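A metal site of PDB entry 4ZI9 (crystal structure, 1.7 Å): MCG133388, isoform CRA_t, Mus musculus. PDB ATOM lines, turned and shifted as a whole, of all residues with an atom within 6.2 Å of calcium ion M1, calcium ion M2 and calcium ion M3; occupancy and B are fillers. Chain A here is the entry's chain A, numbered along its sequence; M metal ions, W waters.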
ATOM      1  N   GLU A  10     -20.480  10.192  13.281  1.00  0.00           N
ATOM      2  CA  GLU A  10     -21.866  10.448  13.647  1.00  0.00           C
ATOM      3  C   GLU A  10     -21.976  10.703  15.159  1.00  0.00           C
ATOM      4  O   GLU A  10     -21.086  10.362  15.921  1.00  0.00           O
ATOM      5  CB  GLU A  10     -22.736   9.247  13.269  1.00  0.00           C
ATOM      6  CG  GLU A  10     -22.206   7.997  13.928  1.00  0.00           C
ATOM      7  CD  GLU A  10     -23.150   6.822  13.845  1.00  0.00           C
ATOM      8  OE1 GLU A  10     -24.380   7.025  13.775  1.00  0.00           O
ATOM      9  OE2 GLU A  10     -22.647   5.684  13.854  1.00  0.00           O
ATOM     10  N   GLU A  11     -23.083  11.318  15.559  1.00  0.00           N
ATOM     11  CA  GLU A  11     -23.472  11.513  16.960  1.00  0.00           C
ATOM     12  C   GLU A  11     -22.557  12.423  17.797  1.00  0.00           C
ATOM     13  O   GLU A  11     -22.597  12.381  19.015  1.00  0.00           O
ATOM     14  CB  GLU A  11     -23.607  10.132  17.665  1.00  0.00           C
ATOM     15  CG  GLU A  11     -24.393   9.070  16.855  1.00  0.00           C
ATOM     16  CD  GLU A  11     -25.896   9.302  16.797  1.00  0.00           C
ATOM     17  OE1 GLU A  11     -26.372  10.335  17.312  1.00  0.00           O
ATOM     18  OE2 GLU A  11     -26.606   8.430  16.247  1.00  0.00           O
ATOM     19  N   ARG A  62     -28.139  16.801  15.163  1.00  0.00           N
ATOM     20  CA  ARG A  62     -27.793  15.397  15.336  1.00  0.00           C
ATOM     21  C   ARG A  62     -27.476  14.778  13.971  1.00  0.00           C
ATOM     22  O   ARG A  62     -28.274  14.864  13.050  1.00  0.00           O
ATOM     23  CB  ARG A  62     -28.913  14.594  16.020  1.00  0.00           C
ATOM     24  CG  ARG A  62     -28.470  13.164  16.349  1.00  0.00           C
ATOM     25  CD  ARG A  62     -29.577  12.226  16.880  1.00  0.00           C
ATOM     26  NE  ARG A  62     -29.044  10.871  17.001  1.00  0.00           N
ATOM     27  CZ  ARG A  62     -29.776   9.758  17.076  1.00  0.00           C
ATOM     28  NH1 ARG A  62     -31.109   9.825  17.058  1.00  0.00           N
ATOM     29  NH2 ARG A  62     -29.202   8.566  17.167  1.00  0.00           N
ATOM     30  N   ILE A  63     -26.297  14.182  13.842  1.00  0.00           N
ATOM     31  CA  ILE A  63     -25.994  13.398  12.645  1.00  0.00           C
ATOM     32  C   ILE A  63     -25.970  11.905  13.002  1.00  0.00           C
ATOM     33  O   ILE A  63     -25.064  11.424  13.695  1.00  0.00           O
ATOM     34  CB  ILE A  63     -24.649  13.829  12.001  1.00  0.00           C
ATOM     35  CG1 ILE A  63     -24.594  15.359  11.858  1.00  0.00           C
ATOM     36  CG2 ILE A  63     -24.487  13.129  10.642  1.00  0.00           C
ATOM     37  CD1 ILE A  63     -23.295  15.902  11.294  1.00  0.00           C
ATOM     38  N   ASP A  64     -26.986  11.179  12.542  1.00  0.00           N
ATOM     39  CA  ASP A  64     -27.098   9.749  12.801  1.00  0.00           C
ATOM     40  C   ASP A  64     -26.884   8.987  11.500  1.00  0.00           C
ATOM     41  O   ASP A  64     -27.732   9.014  10.619  1.00  0.00           O
ATOM     42  CB  ASP A  64     -28.466   9.415  13.399  1.00  0.00           C
ATOM     43  CG  ASP A  64     -28.726   7.905  13.528  1.00  0.00           C
ATOM     44  OD1 ASP A  64     -27.769   7.101  13.665  1.00  0.00           O
ATOM     45  OD2 ASP A  64     -29.907   7.514  13.474  1.00  0.00           O
ATOM     46  N   ARG A  65     -25.738   8.308  11.378  1.00  0.00           N
ATOM     47  CA  ARG A  65     -25.391   7.558  10.167  1.00  0.00           C
ATOM     48  C   ARG A  65     -26.428   6.494   9.825  1.00  0.00           C
ATOM     49  O   ARG A  65     -26.690   6.214   8.657  1.00  0.00           O
ATOM     50  CB  ARG A  65     -24.006   6.907  10.304  1.00  0.00           C
ATOM     51  CG  ARG A  65     -23.450   6.399   8.960  1.00  0.00           C
ATOM     52  CD  ARG A  65     -22.596   5.174   9.141  1.00  0.00           C
ATOM     53  NE  ARG A  65     -23.413   4.084   9.681  1.00  0.00           N
ATOM     54  CZ  ARG A  65     -24.257   3.368   8.959  1.00  0.00           C
ATOM     55  NH1 ARG A  65     -24.386   3.598   7.657  1.00  0.00           N
ATOM     56  NH2 ARG A  65     -24.982   2.417   9.552  1.00  0.00           N
ATOM     57  N   GLU A  66     -27.016   5.899  10.850  1.00  0.00           N
ATOM     58  CA  GLU A  66     -28.001   4.859  10.606  1.00  0.00           C
ATOM     59  C   GLU A  66     -29.216   5.453   9.894  1.00  0.00           C
ATOM     60  O   GLU A  66     -29.687   4.909   8.904  1.00  0.00           O
ATOM     61  CB  GLU A  66     -28.407   4.169  11.919  1.00  0.00           C
ATOM     62  CG  GLU A  66     -27.434   3.076  12.366  1.00  0.00           C
ATOM     63  CD  GLU A  66     -26.072   3.573  12.830  1.00  0.00           C
ATOM     64  OE1 GLU A  66     -25.963   4.338  13.801  1.00  0.00           O
ATOM     65  OE2 GLU A  66     -25.061   3.130  12.247  1.00  0.00           O
ATOM     66  N   GLU A  67     -29.682   6.605  10.372  1.00  0.00           N
ATOM     67  CA  GLU A  67     -30.815   7.258   9.726  1.00  0.00           C
ATOM     68  C   GLU A  67     -30.506   7.721   8.298  1.00  0.00           C
ATOM     69  O   GLU A  67     -31.362   7.628   7.412  1.00  0.00           O
ATOM     70  CB  GLU A  67     -31.283   8.452  10.552  1.00  0.00           C
ATOM     71  CG  GLU A  67     -32.456   9.188   9.917  1.00  0.00           C
ATOM     72  CD  GLU A  67     -32.728  10.533  10.572  1.00  0.00           C
ATOM     73  OE1 GLU A  67     -32.378  10.697  11.763  1.00  0.00           O
ATOM     74  OE2 GLU A  67     -33.281  11.427   9.889  1.00  0.00           O
ATOM     75  N   ASP A  98     -19.074   5.741  10.770  1.00  0.00           N
ATOM     76  CA  ASP A  98     -19.913   4.899  11.618  1.00  0.00           C
ATOM     77  C   ASP A  98     -19.291   4.735  12.986  1.00  0.00           C
ATOM     78  O   ASP A  98     -18.087   4.529  13.095  1.00  0.00           O
ATOM     79  CB  ASP A  98     -20.106   3.516  10.979  1.00  0.00           C
ATOM     80  CG  ASP A  98     -21.034   2.620  11.772  1.00  0.00           C
ATOM     81  OD1 ASP A  98     -22.147   3.055  12.132  1.00  0.00           O
ATOM     82  OD2 ASP A  98     -20.671   1.439  11.997  1.00  0.00           O
ATOM     83  N   ILE A  99     -20.086   4.837  14.044  1.00  0.00           N
ATOM     84  CA  ILE A  99     -19.586   4.397  15.330  1.00  0.00           C
ATOM     85  C   ILE A  99     -20.459   3.228  15.758  1.00  0.00           C
ATOM     86  O   ILE A  99     -21.561   3.010  15.228  1.00  0.00           O
ATOM     87  CB  ILE A  99     -19.630   5.483  16.405  1.00  0.00           C
ATOM     88  CG1 ILE A  99     -21.068   5.748  16.825  1.00  0.00           C
ATOM     89  CG2 ILE A  99     -18.953   6.775  15.898  1.00  0.00           C
ATOM     90  CD1 ILE A  99     -21.186   6.689  18.009  1.00  0.00           C
ATOM     91  N   ASN A 100     -19.950   2.487  16.725  1.00  0.00           N
ATOM     92  CA  ASN A 100     -20.659   1.304  17.176  1.00  0.00           C
ATOM     93  C   ASN A 100     -21.666   1.661  18.235  1.00  0.00           C
ATOM     94  O   ASN A 100     -21.446   1.369  19.407  1.00  0.00           O
ATOM     95  CB  ASN A 100     -19.666   0.266  17.715  1.00  0.00           C
ATOM     96  CG  ASN A 100     -20.313  -1.110  17.831  1.00  0.00           C
ATOM     97  OD1 ASN A 100     -21.227  -1.403  17.077  1.00  0.00           O
ATOM     98  ND2 ASN A 100     -19.838  -1.935  18.754  1.00  0.00           N
ATOM     99  N   ASP A 101     -22.785   2.277  17.849  1.00  0.00           N
ATOM    100  CA  ASP A 101     -23.791   2.673  18.831  1.00  0.00           C
ATOM    101  C   ASP A 101     -25.079   1.835  18.742  1.00  0.00           C
ATOM    102  O   ASP A 101     -26.143   2.268  19.184  1.00  0.00           O
ATOM    103  CB  ASP A 101     -24.146   4.166  18.701  1.00  0.00           C
ATOM    104  CG  ASP A 101     -24.455   4.601  17.274  1.00  0.00           C
ATOM    105  OD1 ASP A 101     -24.065   3.881  16.329  1.00  0.00           O
ATOM    106  OD2 ASP A 101     -25.063   5.677  17.091  1.00  0.00           O
ATOM    107  N   ASN A 102     -24.967   0.660  18.137  1.00  0.00           N
ATOM    108  CA  ASN A 102     -26.104  -0.244  18.060  1.00  0.00           C
ATOM    109  C   ASN A 102     -25.679  -1.642  18.451  1.00  0.00           C
ATOM    110  O   ASN A 102     -24.581  -2.075  18.125  1.00  0.00           O
ATOM    111  CB  ASN A 102     -26.716  -0.253  16.668  1.00  0.00           C
ATOM    112  CG  ASN A 102     -27.412   1.045  16.345  1.00  0.00           C
ATOM    113  OD1 ASN A 102     -28.590   1.237  16.678  1.00  0.00           O
ATOM    114  ND2 ASN A 102     -26.694   1.954  15.696  1.00  0.00           N
ATOM    115  N   THR A 103     -26.545  -2.320  19.203  1.00  0.00           N
ATOM    116  CA  THR A 103     -26.357  -3.720  19.571  1.00  0.00           C
ATOM    117  C   THR A 103     -27.156  -4.620  18.631  1.00  0.00           C
ATOM    118  O   THR A 103     -28.298  -4.275  18.263  1.00  0.00           O
ATOM    119  CB  THR A 103     -26.786  -3.934  21.031  1.00  0.00           C
ATOM    120  OG1 THR A 103     -25.998  -3.094  21.876  1.00  0.00           O
ATOM    121  CG2 THR A 103     -26.648  -5.401  21.460  1.00  0.00           C
ATOM    122  N   PRO A 104     -26.599  -5.778  18.235  1.00  0.00           N
ATOM    123  CA  PRO A 104     -27.415  -6.707  17.438  1.00  0.00           C
ATOM    124  C   PRO A 104     -28.745  -7.022  18.138  1.00  0.00           C
ATOM    125  O   PRO A 104     -28.776  -7.315  19.322  1.00  0.00           O
ATOM    126  CB  PRO A 104     -26.530  -7.960  17.335  1.00  0.00           C
ATOM    127  CG  PRO A 104     -25.143  -7.455  17.521  1.00  0.00           C
ATOM    128  CD  PRO A 104     -25.237  -6.299  18.477  1.00  0.00           C
ATOM    129  N   ASP A 132     -27.824  -6.061  13.232  1.00  0.00           N
ATOM    130  CA  ASP A 132     -27.123  -4.893  13.770  1.00  0.00           C
ATOM    131  C   ASP A 132     -27.223  -3.708  12.804  1.00  0.00           C
ATOM    132  O   ASP A 132     -26.880  -3.836  11.635  1.00  0.00           O
ATOM    133  CB  ASP A 132     -25.653  -5.260  14.008  1.00  0.00           C
ATOM    134  CG  ASP A 132     -24.923  -4.267  14.902  1.00  0.00           C
ATOM    135  OD1 ASP A 132     -24.938  -3.046  14.616  1.00  0.00           O
ATOM    136  OD2 ASP A 132     -24.336  -4.704  15.896  1.00  0.00           O
ATOM    137  N   LEU A 133     -27.713  -2.558  13.278  1.00  0.00           N
ATOM    138  CA  LEU A 133     -27.927  -1.382  12.425  1.00  0.00           C
ATOM    139  C   LEU A 133     -26.646  -0.700  11.974  1.00  0.00           C
ATOM    140  O   LEU A 133     -26.646   0.089  11.019  1.00  0.00           O
ATOM    141  CB  LEU A 133     -28.801  -0.364  13.134  1.00  0.00           C
ATOM    142  CG  LEU A 133     -30.228  -0.834  13.399  1.00  0.00           C
ATOM    143  CD1 LEU A 133     -31.015   0.260  14.109  1.00  0.00           C
ATOM    144  CD2 LEU A 133     -30.895  -1.220  12.086  1.00  0.00           C
ATOM    145  N   ASP A 134     -25.553  -0.977  12.678  1.00  0.00           N
ATOM    146  CA  ASP A 134     -24.255  -0.417  12.299  1.00  0.00           C
ATOM    147  C   ASP A 134     -23.743  -1.089  11.028  1.00  0.00           C
ATOM    148  O   ASP A 134     -24.419  -1.940  10.435  1.00  0.00           O
ATOM    149  CB  ASP A 134     -23.262  -0.563  13.439  1.00  0.00           C
ATOM    150  CG  ASP A 134     -23.732   0.135  14.697  1.00  0.00           C
ATOM    151  OD1 ASP A 134     -24.297   1.246  14.603  1.00  0.00           O
ATOM    152  OD2 ASP A 134     -23.513  -0.413  15.797  1.00  0.00           O
ATOM    153  N   VAL A 135     -22.563  -0.689  10.562  1.00  0.00           N
ATOM    154  CA  VAL A 135     -22.019  -1.262   9.353  1.00  0.00           C
ATOM    155  C   VAL A 135     -20.599  -1.735   9.564  1.00  0.00           C
ATOM    156  O   VAL A 135     -19.973  -1.409  10.573  1.00  0.00           O
ATOM    157  CB  VAL A 135     -22.041  -0.269   8.184  1.00  0.00           C
ATOM    158  CG1 VAL A 135     -23.476  -0.035   7.745  1.00  0.00           C
ATOM    159  CG2 VAL A 135     -21.372   1.046   8.588  1.00  0.00           C
ATOM    160  N   ASN A 138     -18.622  -3.028  12.814  1.00  0.00           N
ATOM    161  CA  ASN A 138     -19.575  -2.755  13.880  1.00  0.00           C
ATOM    162  C   ASN A 138     -20.874  -3.529  13.714  1.00  0.00           C
ATOM    163  O   ASN A 138     -21.767  -3.433  14.568  1.00  0.00           O
ATOM    164  CB  ASN A 138     -19.867  -1.263  13.963  1.00  0.00           C
ATOM    165  CG  ASN A 138     -18.649  -0.467  14.344  1.00  0.00           C
ATOM    166  OD1 ASN A 138     -17.813  -0.946  15.126  1.00  0.00           O
ATOM    167  ND2 ASN A 138     -18.515   0.737  13.784  1.00  0.00           N
ATOM    168  N   SER A 139     -21.007  -4.276  12.632  1.00  0.00           N
ATOM    169  CA  SER A 139     -22.209  -5.093  12.488  1.00  0.00           C
ATOM    170  C   SER A 139     -21.995  -6.511  13.027  1.00  0.00           C
ATOM    171  O   SER A 139     -20.935  -6.850  13.582  1.00  0.00           O
ATOM    172  CB  SER A 139     -22.672  -5.131  11.021  1.00  0.00           C
ATOM    173  OG  SER A 139     -21.624  -5.546  10.176  1.00  0.00           O
ATOM    174  N   LEU A 140     -23.026  -7.332  12.862  1.00  0.00           N
ATOM    175  CA  LEU A 140     -23.038  -8.700  13.380  1.00  0.00           C
ATOM    176  C   LEU A 140     -21.797  -9.466  12.923  1.00  0.00           C
ATOM    177  O   LEU A 140     -21.493  -9.495  11.741  1.00  0.00           O
ATOM    178  CB  LEU A 140     -24.296  -9.422  12.917  1.00  0.00           C
ATOM    179  CG  LEU A 140     -24.491 -10.869  13.406  1.00  0.00           C
ATOM    180  CD1 LEU A 140     -24.634 -10.891  14.896  1.00  0.00           C
ATOM    181  CD2 LEU A 140     -25.717 -11.480  12.756  1.00  0.00           C
ATOM    182  N   ASP A 189     -21.417  -8.084  17.893  1.00  0.00           N
ATOM    183  CA  ASP A 189     -20.833  -7.416  16.745  1.00  0.00           C
ATOM    184  C   ASP A 189     -19.314  -7.448  16.900  1.00  0.00           C
ATOM    185  O   ASP A 189     -18.800  -8.133  17.777  1.00  0.00           O
ATOM    186  CB  ASP A 189     -21.357  -5.973  16.591  1.00  0.00           C
ATOM    187  CG  ASP A 189     -21.101  -5.080  17.812  1.00  0.00           C
ATOM    188  OD1 ASP A 189     -20.120  -5.305  18.559  1.00  0.00           O
ATOM    189  OD2 ASP A 189     -21.884  -4.121  17.997  1.00  0.00           O
ATOM    190  N   GLY A 190     -18.589  -6.700  16.071  1.00  0.00           N
ATOM    191  CA  GLY A 190     -17.144  -6.742  16.153  1.00  0.00           C
ATOM    192  C   GLY A 190     -16.494  -5.457  16.638  1.00  0.00           C
ATOM    193  O   GLY A 190     -15.322  -5.188  16.356  1.00  0.00           O
ATOM    194  N   GLY A 191     -17.249  -4.649  17.394  1.00  0.00           N
ATOM    195  CA  GLY A 191     -16.726  -3.395  17.914  1.00  0.00           C
ATOM    196  C   GLY A 191     -15.784  -3.648  19.079  1.00  0.00           C
ATOM    197  O   GLY A 191     -15.498  -4.798  19.413  1.00  0.00           O
ATOM    198  N   HIS A 195     -20.597  -5.376  21.476  1.00  0.00           N
ATOM    199  CA  HIS A 195     -21.988  -5.375  21.915  1.00  0.00           C
ATOM    200  C   HIS A 195     -22.592  -6.730  21.593  1.00  0.00           C
ATOM    201  O   HIS A 195     -22.317  -7.278  20.532  1.00  0.00           O
ATOM    202  CB  HIS A 195     -22.787  -4.279  21.228  1.00  0.00           C
ATOM    203  CG  HIS A 195     -22.367  -2.901  21.635  1.00  0.00           C
ATOM    204  ND1 HIS A 195     -23.010  -1.766  21.204  1.00  0.00           N
ATOM    205  CD2 HIS A 195     -21.359  -2.491  22.445  1.00  0.00           C
ATOM    206  CE1 HIS A 195     -22.415  -0.705  21.719  1.00  0.00           C
ATOM    207  NE2 HIS A 195     -21.411  -1.112  22.472  1.00  0.00           N
HETATM  208 CA    CA M   1     -23.037  -2.709  16.468  1.00  0.00          CA
HETATM  209 CA    CA M   2     -23.629   3.510  14.034  1.00  0.00          CA
HETATM  210 CA    CA M   3     -26.240   6.289  15.092  1.00  0.00          CA
HETATM  211  O   HOH W   1     -28.016   5.034  16.377  1.00  0.00           O
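Calcium ion M3 is bound by OD1 of Asp 64, at 2.2 Å.
Calcium ion M3 is bound by OE1 of Glu 66 (2.4 Å).
The side-chain carboxylate (OE1) of Glu 10 is bound to calcium ion M3 (2.4 Å).
The side-chain carboxylate (OD2) of Asp 101 binds calcium ion M3 (2.4 Å).
Calcium ion M3 is bound by OE2 of Glu 11 (2.5 Å).
Calcium ion M3 is bound by water W1, at 2.5 Å.
Calcium ion M1 is bound by OD1 of Asn 100 (2.3 Å), O of Asn 102 (2.4 Å), OD2 of Asp 189 (2.4 Å), O of Asn 138 (2.4 Å), OD2 of Asp 134 (2.4 Å), OD2 of Asp 132 (2.4 Å) and OD1 of Asp 132 (2.7 Å).
Of the 26 residues printed, 5 come within 4 Å of calcium ion M3.
OE2 of Glu 66 sits close to NH2 of Arg 65, at 2.8 Å.
The side-chain carboxylate (OD1) of Asp 189 lies within hydrogen-bond range of the backbone NH (N) of Gly 191, 3.2 Å away.
O of Asn 102 lies close to ND1 of His 195 (3.5 Å).
The backbone NH of Arg 65 sits close to the side-chain carboxylate of Glu 10 (3.0 Å).
N of Glu 67 lies within hydrogen-bond range of OD2 of Asp 64.
The backbone NH of Glu 11 lies within hydrogen-bond range of the backbone carbonyl oxygen of Ile 63, at 2.7 Å.
The guanidinium group (NH2) of Arg 62 lies within salt-bridge range of the side-chain carboxylate (OD2) of Asp 64 (3.9 Å).
OE1 of Glu 11 is in salt-bridge range of NE of Arg 62, at 2.7 Å.
Of the 26 residues printed, 7 come within 4 Å of calcium ion M2.
Within 4 Å of calcium ion M1: Asn 100, Asn 102, Asp 132, Asp 134, Asn 138 and Asp 189.
The nearest printed residue that does not touch calcium ion M1 is Thr 103 (4.5 Å).
Calcium ion M2 is bound by the side-chain carboxylate (OE2) of Glu 66 (2.3 Å), the side-chain carboxylate (OD1) of Asp 101 (2.4 Å), the side-chain carboxylate (OE2) of Glu 10 (2.4 Å), the side-chain carboxylate (OD1) of Asp 134 (2.4 Å), the backbone carbonyl oxygen (O) of Ile 99 (2.4 Å), the side-chain carboxylate (OD1) of Asp 98 (2.5 Å) and the side-chain carboxylate (OE1) of Glu 66 (2.5 Å).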
